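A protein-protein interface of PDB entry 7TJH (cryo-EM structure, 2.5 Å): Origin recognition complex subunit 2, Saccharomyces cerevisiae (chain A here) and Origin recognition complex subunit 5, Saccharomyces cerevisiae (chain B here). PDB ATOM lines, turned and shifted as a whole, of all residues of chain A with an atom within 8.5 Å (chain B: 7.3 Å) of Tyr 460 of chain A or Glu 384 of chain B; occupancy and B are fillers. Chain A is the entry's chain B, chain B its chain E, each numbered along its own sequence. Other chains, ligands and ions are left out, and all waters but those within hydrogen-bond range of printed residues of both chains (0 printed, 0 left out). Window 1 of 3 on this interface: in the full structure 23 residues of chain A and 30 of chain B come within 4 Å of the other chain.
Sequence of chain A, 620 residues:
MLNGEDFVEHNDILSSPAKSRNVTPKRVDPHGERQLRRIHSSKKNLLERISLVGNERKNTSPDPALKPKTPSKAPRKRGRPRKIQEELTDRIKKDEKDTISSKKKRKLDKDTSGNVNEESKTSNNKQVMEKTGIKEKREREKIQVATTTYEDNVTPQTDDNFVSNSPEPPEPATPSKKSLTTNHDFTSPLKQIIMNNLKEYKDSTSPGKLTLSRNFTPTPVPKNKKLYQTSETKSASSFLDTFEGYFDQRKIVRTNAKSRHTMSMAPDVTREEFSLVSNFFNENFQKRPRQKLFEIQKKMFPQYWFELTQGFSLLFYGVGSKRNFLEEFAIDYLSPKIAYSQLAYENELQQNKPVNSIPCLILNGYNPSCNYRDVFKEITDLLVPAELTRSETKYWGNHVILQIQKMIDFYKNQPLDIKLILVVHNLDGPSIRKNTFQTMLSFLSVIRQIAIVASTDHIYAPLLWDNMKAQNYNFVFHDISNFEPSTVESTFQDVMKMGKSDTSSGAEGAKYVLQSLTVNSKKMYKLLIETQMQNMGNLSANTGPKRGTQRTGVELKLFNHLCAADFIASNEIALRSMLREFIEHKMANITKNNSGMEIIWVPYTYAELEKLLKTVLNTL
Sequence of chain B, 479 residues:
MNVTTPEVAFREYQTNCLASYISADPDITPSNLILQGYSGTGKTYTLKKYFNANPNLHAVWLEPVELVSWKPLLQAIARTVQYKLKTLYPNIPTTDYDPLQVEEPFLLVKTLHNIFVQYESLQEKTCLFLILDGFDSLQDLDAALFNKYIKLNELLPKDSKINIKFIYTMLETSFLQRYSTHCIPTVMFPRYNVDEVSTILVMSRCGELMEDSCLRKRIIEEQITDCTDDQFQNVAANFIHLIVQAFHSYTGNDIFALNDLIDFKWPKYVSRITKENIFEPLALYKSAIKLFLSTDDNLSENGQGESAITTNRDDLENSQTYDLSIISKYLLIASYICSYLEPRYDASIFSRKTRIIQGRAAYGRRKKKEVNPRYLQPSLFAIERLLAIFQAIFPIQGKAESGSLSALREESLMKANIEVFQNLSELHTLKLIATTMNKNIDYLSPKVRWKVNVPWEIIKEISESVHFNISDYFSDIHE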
ATOM      1  N   THR A 242      20.550  -6.002  42.536  1.00  0.00           N
ATOM      2  CA  THR A 242      19.275  -5.470  42.044  1.00  0.00           C
ATOM      3  C   THR A 242      19.270  -3.943  41.871  1.00  0.00           C
ATOM      4  O   THR A 242      20.324  -3.290  41.943  1.00  0.00           O
ATOM      5  CB  THR A 242      18.097  -6.006  42.908  1.00  0.00           C
ATOM      6  OG1 THR A 242      16.902  -6.025  42.122  1.00  0.00           O
ATOM      7  CG2 THR A 242      17.809  -5.237  44.220  1.00  0.00           C
ATOM      8  N   PHE A 243      18.095  -3.372  41.563  1.00  0.00           N
ATOM      9  CA  PHE A 243      17.975  -1.929  41.365  1.00  0.00           C
ATOM     10  C   PHE A 243      18.300  -1.149  42.636  1.00  0.00           C
ATOM     11  O   PHE A 243      18.722   0.009  42.555  1.00  0.00           O
ATOM     12  CB  PHE A 243      16.574  -1.583  40.839  1.00  0.00           C
ATOM     13  CG  PHE A 243      15.452  -1.806  41.833  1.00  0.00           C
ATOM     14  CD1 PHE A 243      14.823  -3.040  41.918  1.00  0.00           C
ATOM     15  CD2 PHE A 243      14.985  -0.767  42.633  1.00  0.00           C
ATOM     16  CE1 PHE A 243      13.785  -3.245  42.812  1.00  0.00           C
ATOM     17  CE2 PHE A 243      13.952  -0.968  43.531  1.00  0.00           C
ATOM     18  CZ  PHE A 243      13.349  -2.208  43.616  1.00  0.00           C
ATOM     19  N   TYR A 246      21.946  -0.797  42.356  1.00  0.00           N
ATOM     20  CA  TYR A 246      22.198   0.169  41.285  1.00  0.00           C
ATOM     21  C   TYR A 246      22.028   1.603  41.773  1.00  0.00           C
ATOM     22  O   TYR A 246      22.876   2.464  41.511  1.00  0.00           O
ATOM     23  CB  TYR A 246      21.268  -0.095  40.098  1.00  0.00           C
ATOM     24  CG  TYR A 246      21.496   0.849  38.935  1.00  0.00           C
ATOM     25  CD1 TYR A 246      22.544   0.641  38.045  1.00  0.00           C
ATOM     26  CD2 TYR A 246      20.664   1.950  38.723  1.00  0.00           C
ATOM     27  CE1 TYR A 246      22.761   1.497  36.982  1.00  0.00           C
ATOM     28  CE2 TYR A 246      20.878   2.816  37.667  1.00  0.00           C
ATOM     29  CZ  TYR A 246      21.925   2.581  36.798  1.00  0.00           C
ATOM     30  OH  TYR A 246      22.142   3.436  35.748  1.00  0.00           O
ATOM     31  N   PHE A 247      20.941   1.880  42.489  1.00  0.00           N
ATOM     32  CA  PHE A 247      20.713   3.238  42.969  1.00  0.00           C
ATOM     33  C   PHE A 247      21.599   3.585  44.160  1.00  0.00           C
ATOM     34  O   PHE A 247      22.004   4.743  44.301  1.00  0.00           O
ATOM     35  CB  PHE A 247      19.239   3.432  43.325  1.00  0.00           C
ATOM     36  CG  PHE A 247      18.318   3.347  42.142  1.00  0.00           C
ATOM     37  CD1 PHE A 247      18.682   3.905  40.927  1.00  0.00           C
ATOM     38  CD2 PHE A 247      17.090   2.717  42.244  1.00  0.00           C
ATOM     39  CE1 PHE A 247      17.840   3.827  39.831  1.00  0.00           C
ATOM     40  CE2 PHE A 247      16.245   2.630  41.154  1.00  0.00           C
ATOM     41  CZ  PHE A 247      16.618   3.191  39.946  1.00  0.00           C
ATOM     42  N   ARG A 250      25.452   4.331  43.082  1.00  0.00           N
ATOM     43  CA  ARG A 250      25.664   5.520  42.258  1.00  0.00           C
ATOM     44  C   ARG A 250      25.350   6.791  43.044  1.00  0.00           C
ATOM     45  O   ARG A 250      24.425   7.540  42.734  1.00  0.00           O
ATOM     46  CB  ARG A 250      24.831   5.437  40.986  1.00  0.00           C
ATOM     47  CG  ARG A 250      25.216   4.285  40.088  1.00  0.00           C
ATOM     48  CD  ARG A 250      24.225   4.117  38.964  1.00  0.00           C
ATOM     49  NE  ARG A 250      24.263   5.236  38.033  1.00  0.00           N
ATOM     50  CZ  ARG A 250      24.902   5.221  36.873  1.00  0.00           C
ATOM     51  NH1 ARG A 250      25.573   4.157  36.467  1.00  0.00           N
ATOM     52  NH2 ARG A 250      24.873   6.304  36.102  1.00  0.00           N
ATOM     53  N   ASP A 428      28.432 -11.494  18.383  1.00  0.00           N
ATOM     54  CA  ASP A 428      28.350 -10.165  18.959  1.00  0.00           C
ATOM     55  C   ASP A 428      29.611  -9.319  18.775  1.00  0.00           C
ATOM     56  O   ASP A 428      29.741  -8.286  19.434  1.00  0.00           O
ATOM     57  CB  ASP A 428      28.034 -10.320  20.442  1.00  0.00           C
ATOM     58  CG  ASP A 428      29.222 -10.849  21.223  1.00  0.00           C
ATOM     59  OD1 ASP A 428      29.984 -11.677  20.677  1.00  0.00           O
ATOM     60  OD2 ASP A 428      29.417 -10.449  22.374  1.00  0.00           O
ATOM     61  N   THR A 456      28.432 -15.955  21.688  1.00  0.00           N
ATOM     62  CA  THR A 456      28.341 -14.549  22.065  1.00  0.00           C
ATOM     63  C   THR A 456      29.163 -14.300  23.319  1.00  0.00           C
ATOM     64  O   THR A 456      29.316 -15.183  24.163  1.00  0.00           O
ATOM     65  CB  THR A 456      26.890 -14.088  22.327  1.00  0.00           C
ATOM     66  OG1 THR A 456      26.292 -14.909  23.337  1.00  0.00           O
ATOM     67  CG2 THR A 456      26.053 -14.141  21.061  1.00  0.00           C
ATOM     68  N   ASP A 457      29.674 -13.080  23.446  1.00  0.00           N
ATOM     69  CA  ASP A 457      30.504 -12.694  24.578  1.00  0.00           C
ATOM     70  C   ASP A 457      29.958 -11.526  25.385  1.00  0.00           C
ATOM     71  O   ASP A 457      30.237 -11.450  26.584  1.00  0.00           O
ATOM     72  CB  ASP A 457      31.921 -12.338  24.101  1.00  0.00           C
ATOM     73  CG  ASP A 457      32.848 -13.531  24.092  1.00  0.00           C
ATOM     74  OD1 ASP A 457      32.545 -14.526  24.782  1.00  0.00           O
ATOM     75  OD2 ASP A 457      33.879 -13.476  23.392  1.00  0.00           O
ATOM     76  N   HIS A 458      29.204 -10.616  24.773  1.00  0.00           N
ATOM     77  CA  HIS A 458      28.708  -9.437  25.473  1.00  0.00           C
ATOM     78  C   HIS A 458      27.535  -9.802  26.369  1.00  0.00           C
ATOM     79  O   HIS A 458      26.729 -10.676  26.042  1.00  0.00           O
ATOM     80  CB  HIS A 458      28.284  -8.356  24.474  1.00  0.00           C
ATOM     81  CG  HIS A 458      28.364  -6.961  25.005  1.00  0.00           C
ATOM     82  ND1 HIS A 458      27.338  -6.371  25.711  1.00  0.00           N
ATOM     83  CD2 HIS A 458      29.343  -6.031  24.918  1.00  0.00           C
ATOM     84  CE1 HIS A 458      27.684  -5.141  26.042  1.00  0.00           C
ATOM     85  NE2 HIS A 458      28.898  -4.911  25.573  1.00  0.00           N
ATOM     86  N   ILE A 459      27.439  -9.110  27.505  1.00  0.00           N
ATOM     87  CA  ILE A 459      26.347  -9.332  28.444  1.00  0.00           C
ATOM     88  C   ILE A 459      25.010  -8.825  27.904  1.00  0.00           C
ATOM     89  O   ILE A 459      23.951  -9.240  28.387  1.00  0.00           O
ATOM     90  CB  ILE A 459      26.719  -8.685  29.795  1.00  0.00           C
ATOM     91  CG1 ILE A 459      25.941  -9.315  30.953  1.00  0.00           C
ATOM     92  CG2 ILE A 459      26.548  -7.177  29.744  1.00  0.00           C
ATOM     93  CD1 ILE A 459      26.766  -9.531  32.184  1.00  0.00           C
ATOM     94  N   TYR A 460      25.025  -7.964  26.887  1.00  0.00           N
ATOM     95  CA  TYR A 460      23.818  -7.373  26.325  1.00  0.00           C
ATOM     96  C   TYR A 460      23.490  -7.927  24.940  1.00  0.00           C
ATOM     97  O   TYR A 460      22.715  -7.310  24.210  1.00  0.00           O
ATOM     98  CB  TYR A 460      23.959  -5.852  26.263  1.00  0.00           C
ATOM     99  CG  TYR A 460      23.784  -5.136  27.584  1.00  0.00           C
ATOM    100  CD1 TYR A 460      23.325  -5.806  28.712  1.00  0.00           C
ATOM    101  CD2 TYR A 460      24.085  -3.785  27.702  1.00  0.00           C
ATOM    102  CE1 TYR A 460      23.168  -5.150  29.917  1.00  0.00           C
ATOM    103  CE2 TYR A 460      23.932  -3.119  28.906  1.00  0.00           C
ATOM    104  CZ  TYR A 460      23.473  -3.806  30.007  1.00  0.00           C
ATOM    105  OH  TYR A 460      23.320  -3.146  31.203  1.00  0.00           O
ATOM    106  N   ALA A 461      24.073  -9.073  24.576  1.00  0.00           N
ATOM    107  CA  ALA A 461      23.884  -9.651  23.242  1.00  0.00           C
ATOM    108  C   ALA A 461      22.435  -9.942  22.817  1.00  0.00           C
ATOM    109  O   ALA A 461      22.136  -9.726  21.629  1.00  0.00           O
ATOM    110  CB  ALA A 461      24.753 -10.912  23.109  1.00  0.00           C
ATOM    111  N   PRO A 462      21.501 -10.403  23.675  1.00  0.00           N
ATOM    112  CA  PRO A 462      20.101 -10.539  23.214  1.00  0.00           C
ATOM    113  C   PRO A 462      19.400  -9.236  22.818  1.00  0.00           C
ATOM    114  O   PRO A 462      18.299  -9.307  22.258  1.00  0.00           O
ATOM    115  CB  PRO A 462      19.391 -11.195  24.407  1.00  0.00           C
ATOM    116  CG  PRO A 462      20.315 -11.068  25.544  1.00  0.00           C
ATOM    117  CD  PRO A 462      21.664 -11.138  24.948  1.00  0.00           C
ATOM    118  N   LEU A 463      19.989  -8.063  23.068  1.00  0.00           N
ATOM    119  CA  LEU A 463      19.472  -6.822  22.506  1.00  0.00           C
ATOM    120  C   LEU A 463      19.658  -6.735  20.992  1.00  0.00           C
ATOM    121  O   LEU A 463      19.015  -5.894  20.354  1.00  0.00           O
ATOM    122  CB  LEU A 463      20.140  -5.630  23.205  1.00  0.00           C
ATOM    123  CG  LEU A 463      19.651  -4.189  23.038  1.00  0.00           C
ATOM    124  CD1 LEU A 463      18.209  -4.047  23.481  1.00  0.00           C
ATOM    125  CD2 LEU A 463      20.551  -3.241  23.808  1.00  0.00           C
ATOM    126  N   LEU A 464      20.492  -7.592  20.396  1.00  0.00           N
ATOM    127  CA  LEU A 464      20.669  -7.567  18.948  1.00  0.00           C
ATOM    128  C   LEU A 464      19.452  -8.080  18.182  1.00  0.00           C
ATOM    129  O   LEU A 464      19.305  -7.749  17.002  1.00  0.00           O
ATOM    130  CB  LEU A 464      21.894  -8.390  18.550  1.00  0.00           C
ATOM    131  CG  LEU A 464      23.261  -7.911  19.035  1.00  0.00           C
ATOM    132  CD1 LEU A 464      24.343  -8.853  18.548  1.00  0.00           C
ATOM    133  CD2 LEU A 464      23.536  -6.485  18.585  1.00  0.00           C
ATOM    134  N   TRP A 465      18.585  -8.874  18.805  1.00  0.00           N
ATOM    135  CA  TRP A 465      17.561  -9.622  18.082  1.00  0.00           C
ATOM    136  C   TRP A 465      16.168  -9.200  18.527  1.00  0.00           C
ATOM    137  O   TRP A 465      15.831  -9.301  19.710  1.00  0.00           O
ATOM    138  CB  TRP A 465      17.752 -11.129  18.278  1.00  0.00           C
ATOM    139  CG  TRP A 465      19.189 -11.556  18.210  1.00  0.00           C
ATOM    140  CD1 TRP A 465      20.065 -11.317  17.193  1.00  0.00           C
ATOM    141  CD2 TRP A 465      19.916 -12.292  19.199  1.00  0.00           C
ATOM    142  NE1 TRP A 465      21.289 -11.856  17.487  1.00  0.00           N
ATOM    143  CE2 TRP A 465      21.226 -12.459  18.714  1.00  0.00           C
ATOM    144  CE3 TRP A 465      19.587 -12.826  20.449  1.00  0.00           C
ATOM    145  CZ2 TRP A 465      22.207 -13.139  19.433  1.00  0.00           C
ATOM    146  CZ3 TRP A 465      20.563 -13.497  21.162  1.00  0.00           C
ATOM    147  CH2 TRP A 465      21.856 -13.648  20.653  1.00  0.00           C
ATOM    148  N   CYS B 338      12.531   7.215  32.743  1.00  0.00           N
ATOM    149  CA  CYS B 338      13.966   7.461  32.608  1.00  0.00           C
ATOM    150  C   CYS B 338      14.266   8.678  31.742  1.00  0.00           C
ATOM    151  O   CYS B 338      15.283   9.350  31.949  1.00  0.00           O
ATOM    152  CB  CYS B 338      14.656   6.234  32.015  1.00  0.00           C
ATOM    153  SG  CYS B 338      14.994   4.890  33.148  1.00  0.00           S
ATOM    154  N   PHE B 381      19.320   8.115  28.356  1.00  0.00           N
ATOM    155  CA  PHE B 381      19.639   7.265  29.493  1.00  0.00           C
ATOM    156  C   PHE B 381      20.426   6.046  29.027  1.00  0.00           C
ATOM    157  O   PHE B 381      20.544   5.771  27.831  1.00  0.00           O
ATOM    158  CB  PHE B 381      18.370   6.837  30.255  1.00  0.00           C
ATOM    159  CG  PHE B 381      17.274   6.274  29.378  1.00  0.00           C
ATOM    160  CD1 PHE B 381      17.272   4.934  29.003  1.00  0.00           C
ATOM    161  CD2 PHE B 381      16.226   7.079  28.960  1.00  0.00           C
ATOM    162  CE1 PHE B 381      16.267   4.421  28.209  1.00  0.00           C
ATOM    163  CE2 PHE B 381      15.214   6.567  28.171  1.00  0.00           C
ATOM    164  CZ  PHE B 381      15.236   5.238  27.793  1.00  0.00           C
ATOM    165  N   ALA B 382      20.954   5.306  29.996  1.00  0.00           N
ATOM    166  CA  ALA B 382      21.664   4.058  29.754  1.00  0.00           C
ATOM    167  C   ALA B 382      20.732   2.864  29.941  1.00  0.00           C
ATOM    168  O   ALA B 382      19.619   2.986  30.457  1.00  0.00           O
ATOM    169  CB  ALA B 382      22.878   3.941  30.677  1.00  0.00           C
ATOM    170  N   ILE B 383      21.215   1.694  29.511  1.00  0.00           N
ATOM    171  CA  ILE B 383      20.405   0.477  29.528  1.00  0.00           C
ATOM    172  C   ILE B 383      20.140   0.014  30.956  1.00  0.00           C
ATOM    173  O   ILE B 383      19.011  -0.364  31.297  1.00  0.00           O
ATOM    174  CB  ILE B 383      21.088  -0.623  28.688  1.00  0.00           C
ATOM    175  CG1 ILE B 383      21.136  -0.214  27.214  1.00  0.00           C
ATOM    176  CG2 ILE B 383      20.398  -1.977  28.859  1.00  0.00           C
ATOM    177  CD1 ILE B 383      19.822  -0.377  26.480  1.00  0.00           C
ATOM    178  N   GLU B 384      21.163   0.054  31.816  1.00  0.00           N
ATOM    179  CA  GLU B 384      21.017  -0.467  33.171  1.00  0.00           C
ATOM    180  C   GLU B 384      20.096   0.394  34.029  1.00  0.00           C
ATOM    181  O   GLU B 384      19.415  -0.137  34.911  1.00  0.00           O
ATOM    182  CB  GLU B 384      22.390  -0.619  33.831  1.00  0.00           C
ATOM    183  CG  GLU B 384      22.468  -1.719  34.900  1.00  0.00           C
ATOM    184  CD  GLU B 384      22.629  -3.152  34.366  1.00  0.00           C
ATOM    185  OE1 GLU B 384      22.143  -3.483  33.262  1.00  0.00           O
ATOM    186  OE2 GLU B 384      23.224  -3.975  35.090  1.00  0.00           O
ATOM    187  N   ARG B 385      20.031   1.702  33.763  1.00  0.00           N
ATOM    188  CA  ARG B 385      19.051   2.553  34.433  1.00  0.00           C
ATOM    189  C   ARG B 385      17.623   2.180  34.041  1.00  0.00           C
ATOM    190  O   ARG B 385      16.727   2.127  34.900  1.00  0.00           O
ATOM    191  CB  ARG B 385      19.327   4.017  34.104  1.00  0.00           C
ATOM    192  CG  ARG B 385      18.701   4.988  35.072  1.00  0.00           C
ATOM    193  CD  ARG B 385      18.448   6.323  34.419  1.00  0.00           C
ATOM    194  NE  ARG B 385      17.347   7.028  35.060  1.00  0.00           N
ATOM    195  CZ  ARG B 385      16.897   8.214  34.683  1.00  0.00           C
ATOM    196  NH1 ARG B 385      17.456   8.882  33.688  1.00  0.00           N
ATOM    197  NH2 ARG B 385      15.856   8.744  35.317  1.00  0.00           N
ATOM    198  N   LEU B 386      17.401   1.916  32.748  1.00  0.00           N
ATOM    199  CA  LEU B 386      16.091   1.491  32.268  1.00  0.00           C
ATOM    200  C   LEU B 386      15.702   0.139  32.849  1.00  0.00           C
ATOM    201  O   LEU B 386      14.546  -0.067  33.234  1.00  0.00           O
ATOM    202  CB  LEU B 386      16.089   1.452  30.739  1.00  0.00           C
ATOM    203  CG  LEU B 386      14.993   0.657  30.026  1.00  0.00           C
ATOM    204  CD1 LEU B 386      13.662   1.360  30.130  1.00  0.00           C
ATOM    205  CD2 LEU B 386      15.359   0.437  28.577  1.00  0.00           C
ATOM    206  N   LEU B 387      16.662  -0.784  32.949  1.00  0.00           N
ATOM    207  CA  LEU B 387      16.387  -2.081  33.556  1.00  0.00           C
ATOM    208  C   LEU B 387      16.136  -1.962  35.054  1.00  0.00           C
ATOM    209  O   LEU B 387      15.316  -2.709  35.594  1.00  0.00           O
ATOM    210  CB  LEU B 387      17.539  -3.048  33.283  1.00  0.00           C
ATOM    211  CG  LEU B 387      17.770  -3.426  31.819  1.00  0.00           C
ATOM    212  CD1 LEU B 387      18.889  -4.451  31.710  1.00  0.00           C
ATOM    213  CD2 LEU B 387      16.488  -3.928  31.165  1.00  0.00           C
ATOM    214  N   ALA B 388      16.801  -1.014  35.722  1.00  0.00           N
ATOM    215  CA  ALA B 388      16.558  -0.757  37.139  1.00  0.00           C
ATOM    216  C   ALA B 388      15.137  -0.267  37.381  1.00  0.00           C
ATOM    217  O   ALA B 388      14.433  -0.775  38.262  1.00  0.00           O
ATOM    218  CB  ALA B 388      17.562   0.268  37.663  1.00  0.00           C
ATOM    219  N   ILE B 389      14.697   0.717  36.596  1.00  0.00           N
ATOM    220  CA  ILE B 389      13.353   1.256  36.791  1.00  0.00           C
ATOM    221  C   ILE B 389      12.289   0.249  36.338  1.00  0.00           C
ATOM    222  O   ILE B 389      11.230   0.129  36.975  1.00  0.00           O
ATOM    223  CB  ILE B 389      13.253   2.634  36.106  1.00  0.00           C
ATOM    224  CG1 ILE B 389      14.074   3.637  36.926  1.00  0.00           C
ATOM    225  CG2 ILE B 389      11.806   3.109  35.951  1.00  0.00           C
ATOM    226  CD1 ILE B 389      13.874   5.093  36.587  1.00  0.00           C
ATOM    227  N   PHE B 390      12.581  -0.536  35.292  1.00  0.00           N
ATOM    228  CA  PHE B 390      11.685  -1.611  34.867  1.00  0.00           C
ATOM    229  C   PHE B 390      11.535  -2.676  35.947  1.00  0.00           C
ATOM    230  O   PHE B 390      10.432  -3.183  36.173  1.00  0.00           O
ATOM    231  CB  PHE B 390      12.205  -2.232  33.566  1.00  0.00           C
ATOM    232  CG  PHE B 390      11.512  -3.513  33.169  1.00  0.00           C
ATOM    233  CD1 PHE B 390      10.269  -3.479  32.552  1.00  0.00           C
ATOM    234  CD2 PHE B 390      12.111  -4.746  33.387  1.00  0.00           C
ATOM    235  CE1 PHE B 390       9.632  -4.649  32.181  1.00  0.00           C
ATOM    236  CE2 PHE B 390      11.476  -5.918  33.022  1.00  0.00           C
ATOM    237  CZ  PHE B 390      10.239  -5.870  32.417  1.00  0.00           C
ATOM    238  N   ALA B 416      16.485  -9.529  34.246  1.00  0.00           N
ATOM    239  CA  ALA B 416      16.533  -9.204  32.822  1.00  0.00           C
ATOM    240  C   ALA B 416      16.984 -10.433  32.042  1.00  0.00           C
ATOM    241  O   ALA B 416      18.176 -10.674  31.847  1.00  0.00           O
ATOM    242  CB  ALA B 416      17.456  -8.018  32.578  1.00  0.00           C
ATOM    243  N   PHE B 421      15.023  -8.339  26.824  1.00  0.00           N
ATOM    244  CA  PHE B 421      15.891  -7.727  25.822  1.00  0.00           C
ATOM    245  C   PHE B 421      15.308  -7.841  24.419  1.00  0.00           C
ATOM    246  O   PHE B 421      15.479  -6.927  23.605  1.00  0.00           O
ATOM    247  CB  PHE B 421      17.282  -8.359  25.880  1.00  0.00           C
ATOM    248  CG  PHE B 421      18.132  -7.836  26.996  1.00  0.00           C
ATOM    249  CD1 PHE B 421      18.878  -6.679  26.833  1.00  0.00           C
ATOM    250  CD2 PHE B 421      18.184  -8.495  28.213  1.00  0.00           C
ATOM    251  CE1 PHE B 421      19.662  -6.192  27.864  1.00  0.00           C
ATOM    252  CE2 PHE B 421      18.963  -8.015  29.250  1.00  0.00           C
ATOM    253  CZ  PHE B 421      19.704  -6.863  29.074  1.00  0.00           C
ATOM    254  N   TYR B 443      24.423  -1.393  18.815  1.00  0.00           N
ATOM    255  CA  TYR B 443      23.550  -1.593  19.972  1.00  0.00           C
ATOM    256  C   TYR B 443      24.351  -1.815  21.250  1.00  0.00           C
ATOM    257  O   TYR B 443      23.952  -1.364  22.328  1.00  0.00           O
ATOM    258  CB  TYR B 443      22.628  -2.786  19.729  1.00  0.00           C
ATOM    259  CG  TYR B 443      21.302  -2.470  19.078  1.00  0.00           C
ATOM    260  CD1 TYR B 443      20.698  -1.227  19.233  1.00  0.00           C
ATOM    261  CD2 TYR B 443      20.643  -3.431  18.321  1.00  0.00           C
ATOM    262  CE1 TYR B 443      19.479  -0.949  18.638  1.00  0.00           C
ATOM    263  CE2 TYR B 443      19.426  -3.167  17.727  1.00  0.00           C
ATOM    264  CZ  TYR B 443      18.848  -1.926  17.887  1.00  0.00           C
ATOM    265  OH  TYR B 443      17.637  -1.669  17.290  1.00  0.00           O
ATOM    266  N   LEU B 444      25.485  -2.498  21.144  1.00  0.00           N
ATOM    267  CA  LEU B 444      26.285  -2.892  22.293  1.00  0.00           C
ATOM    268  C   LEU B 444      27.295  -1.833  22.714  1.00  0.00           C
ATOM    269  O   LEU B 444      28.059  -2.069  23.653  1.00  0.00           O
ATOM    270  CB  LEU B 444      27.008  -4.207  21.984  1.00  0.00           C
ATOM    271  CG  LEU B 444      26.076  -5.345  21.556  1.00  0.00           C
ATOM    272  CD1 LEU B 444      26.850  -6.609  21.216  1.00  0.00           C
ATOM    273  CD2 LEU B 444      25.053  -5.619  22.633  1.00  0.00           C
ATOM    274  N   SER B 445      27.323  -0.688  22.045  1.00  0.00           N
ATOM    275  CA  SER B 445      28.263   0.366  22.409  1.00  0.00           C
ATOM    276  C   SER B 445      27.813   1.052  23.693  1.00  0.00           C
ATOM    277  O   SER B 445      26.643   1.438  23.802  1.00  0.00           O
ATOM    278  CB  SER B 445      28.383   1.389  21.283  1.00  0.00           C
ATOM    279  OG  SER B 445      29.049   2.559  21.723  1.00  0.00           O
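OD2 of Asp 428 of chain A lies within hydrogen-bond range of N of Asp 457 of chain A (2.9 Å).
N of His 458 of chain A is in hydrogen-bond range of OD2 of Asp 428 of chain A (2.4 Å).
The backbone NH (N) of Tyr 460 of chain A is in hydrogen-bond range of a ring nitrogen (ND1) of His 458 of chain A (3.0 Å).
O of Cys 338 of chain B sits at hydrogen-bond distance from NH1 of Arg 385 of chain B (2.8 Å).
OH of Tyr 246 of chain A sits close to N of Arg 385 of chain B (3.4 Å).
OE1 of Glu 384 of chain B lies close to OH of Tyr 460 of chain A (2.4 Å).
Of the printed residues of chain B, Phe 247 of chain A touches Ala 388 and Ile 389.
Of the printed residues of chain B, His 458 of chain A touches Leu 444.
Of chain B, only Ile 383, Glu 384, Phe 421 and Leu 444 come within 4 Å of Tyr 460 of chain A.
Phe 381 of chain B touches none of the printed residues of chain A.
Printed residues of chain A within 4 Å of Ile 383 of chain B: Tyr 460 (3.7 Å) and Leu 463 (3.98 Å).
Of chain A, only Tyr 246 (3.8 Å) and Tyr 460 (2.4 Å) come within 4 Å of Glu 384 of chain B.
Printed residues of chain A within 4 Å of Ile 389 of chain B: Phe 247.
Printed residues of chain A within 4 Å of Leu 444 of chain B: Asp 428 (3.8 Å), His 458 (3.5 Å) and Tyr 460 (3.3 Å).
The nearest residue of chain B that does not touch Tyr 460 of chain A is Leu 387 of chain B (4.6 Å).
The nearest residue of chain A that does not touch Glu 384 of chain B is Arg 250 of chain A (6.3 Å).
Phe 243 of chain A touches Ala 388 of chain B.
Ala 388 of chain B touches Tyr 246 of chain A (CB to CD2, 3.7 Å).
Ala 388 of chain B touches Phe 247 of chain A.
CD1 of Leu 444 of chain B touches O of Asp 428 of chain A, 3.8 Å away.
NE2 of His 458 of chain A touches O of Leu 444 of chain B (3.5 Å).
CE2 of Tyr 460 of chain A touches CG2 of Ile 383 of chain B (3.7 Å).
Tyr 460 of chain A touches Leu 444 of chain B (O to CD2, 3.3 Å).
Phe 421 of chain B touches Leu 463 of chain A.
CD2 of Tyr 443 of chain B touches O of Leu 463 of chain A (3.6 Å).
Leu 464 of chain A touches Tyr 443 of chain B (CD2 to CB, 3.98 Å).
Of the 16 printed residues of chain A, 9 touch a printed residue of chain B.
Of the 16 printed residues of chain B, 8 touch a printed residue of chain A.
Among the printed residues, no Asp or Glu carboxylate lies within 4 Å of a Lys or Arg side-chain nitrogen of the other chain.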
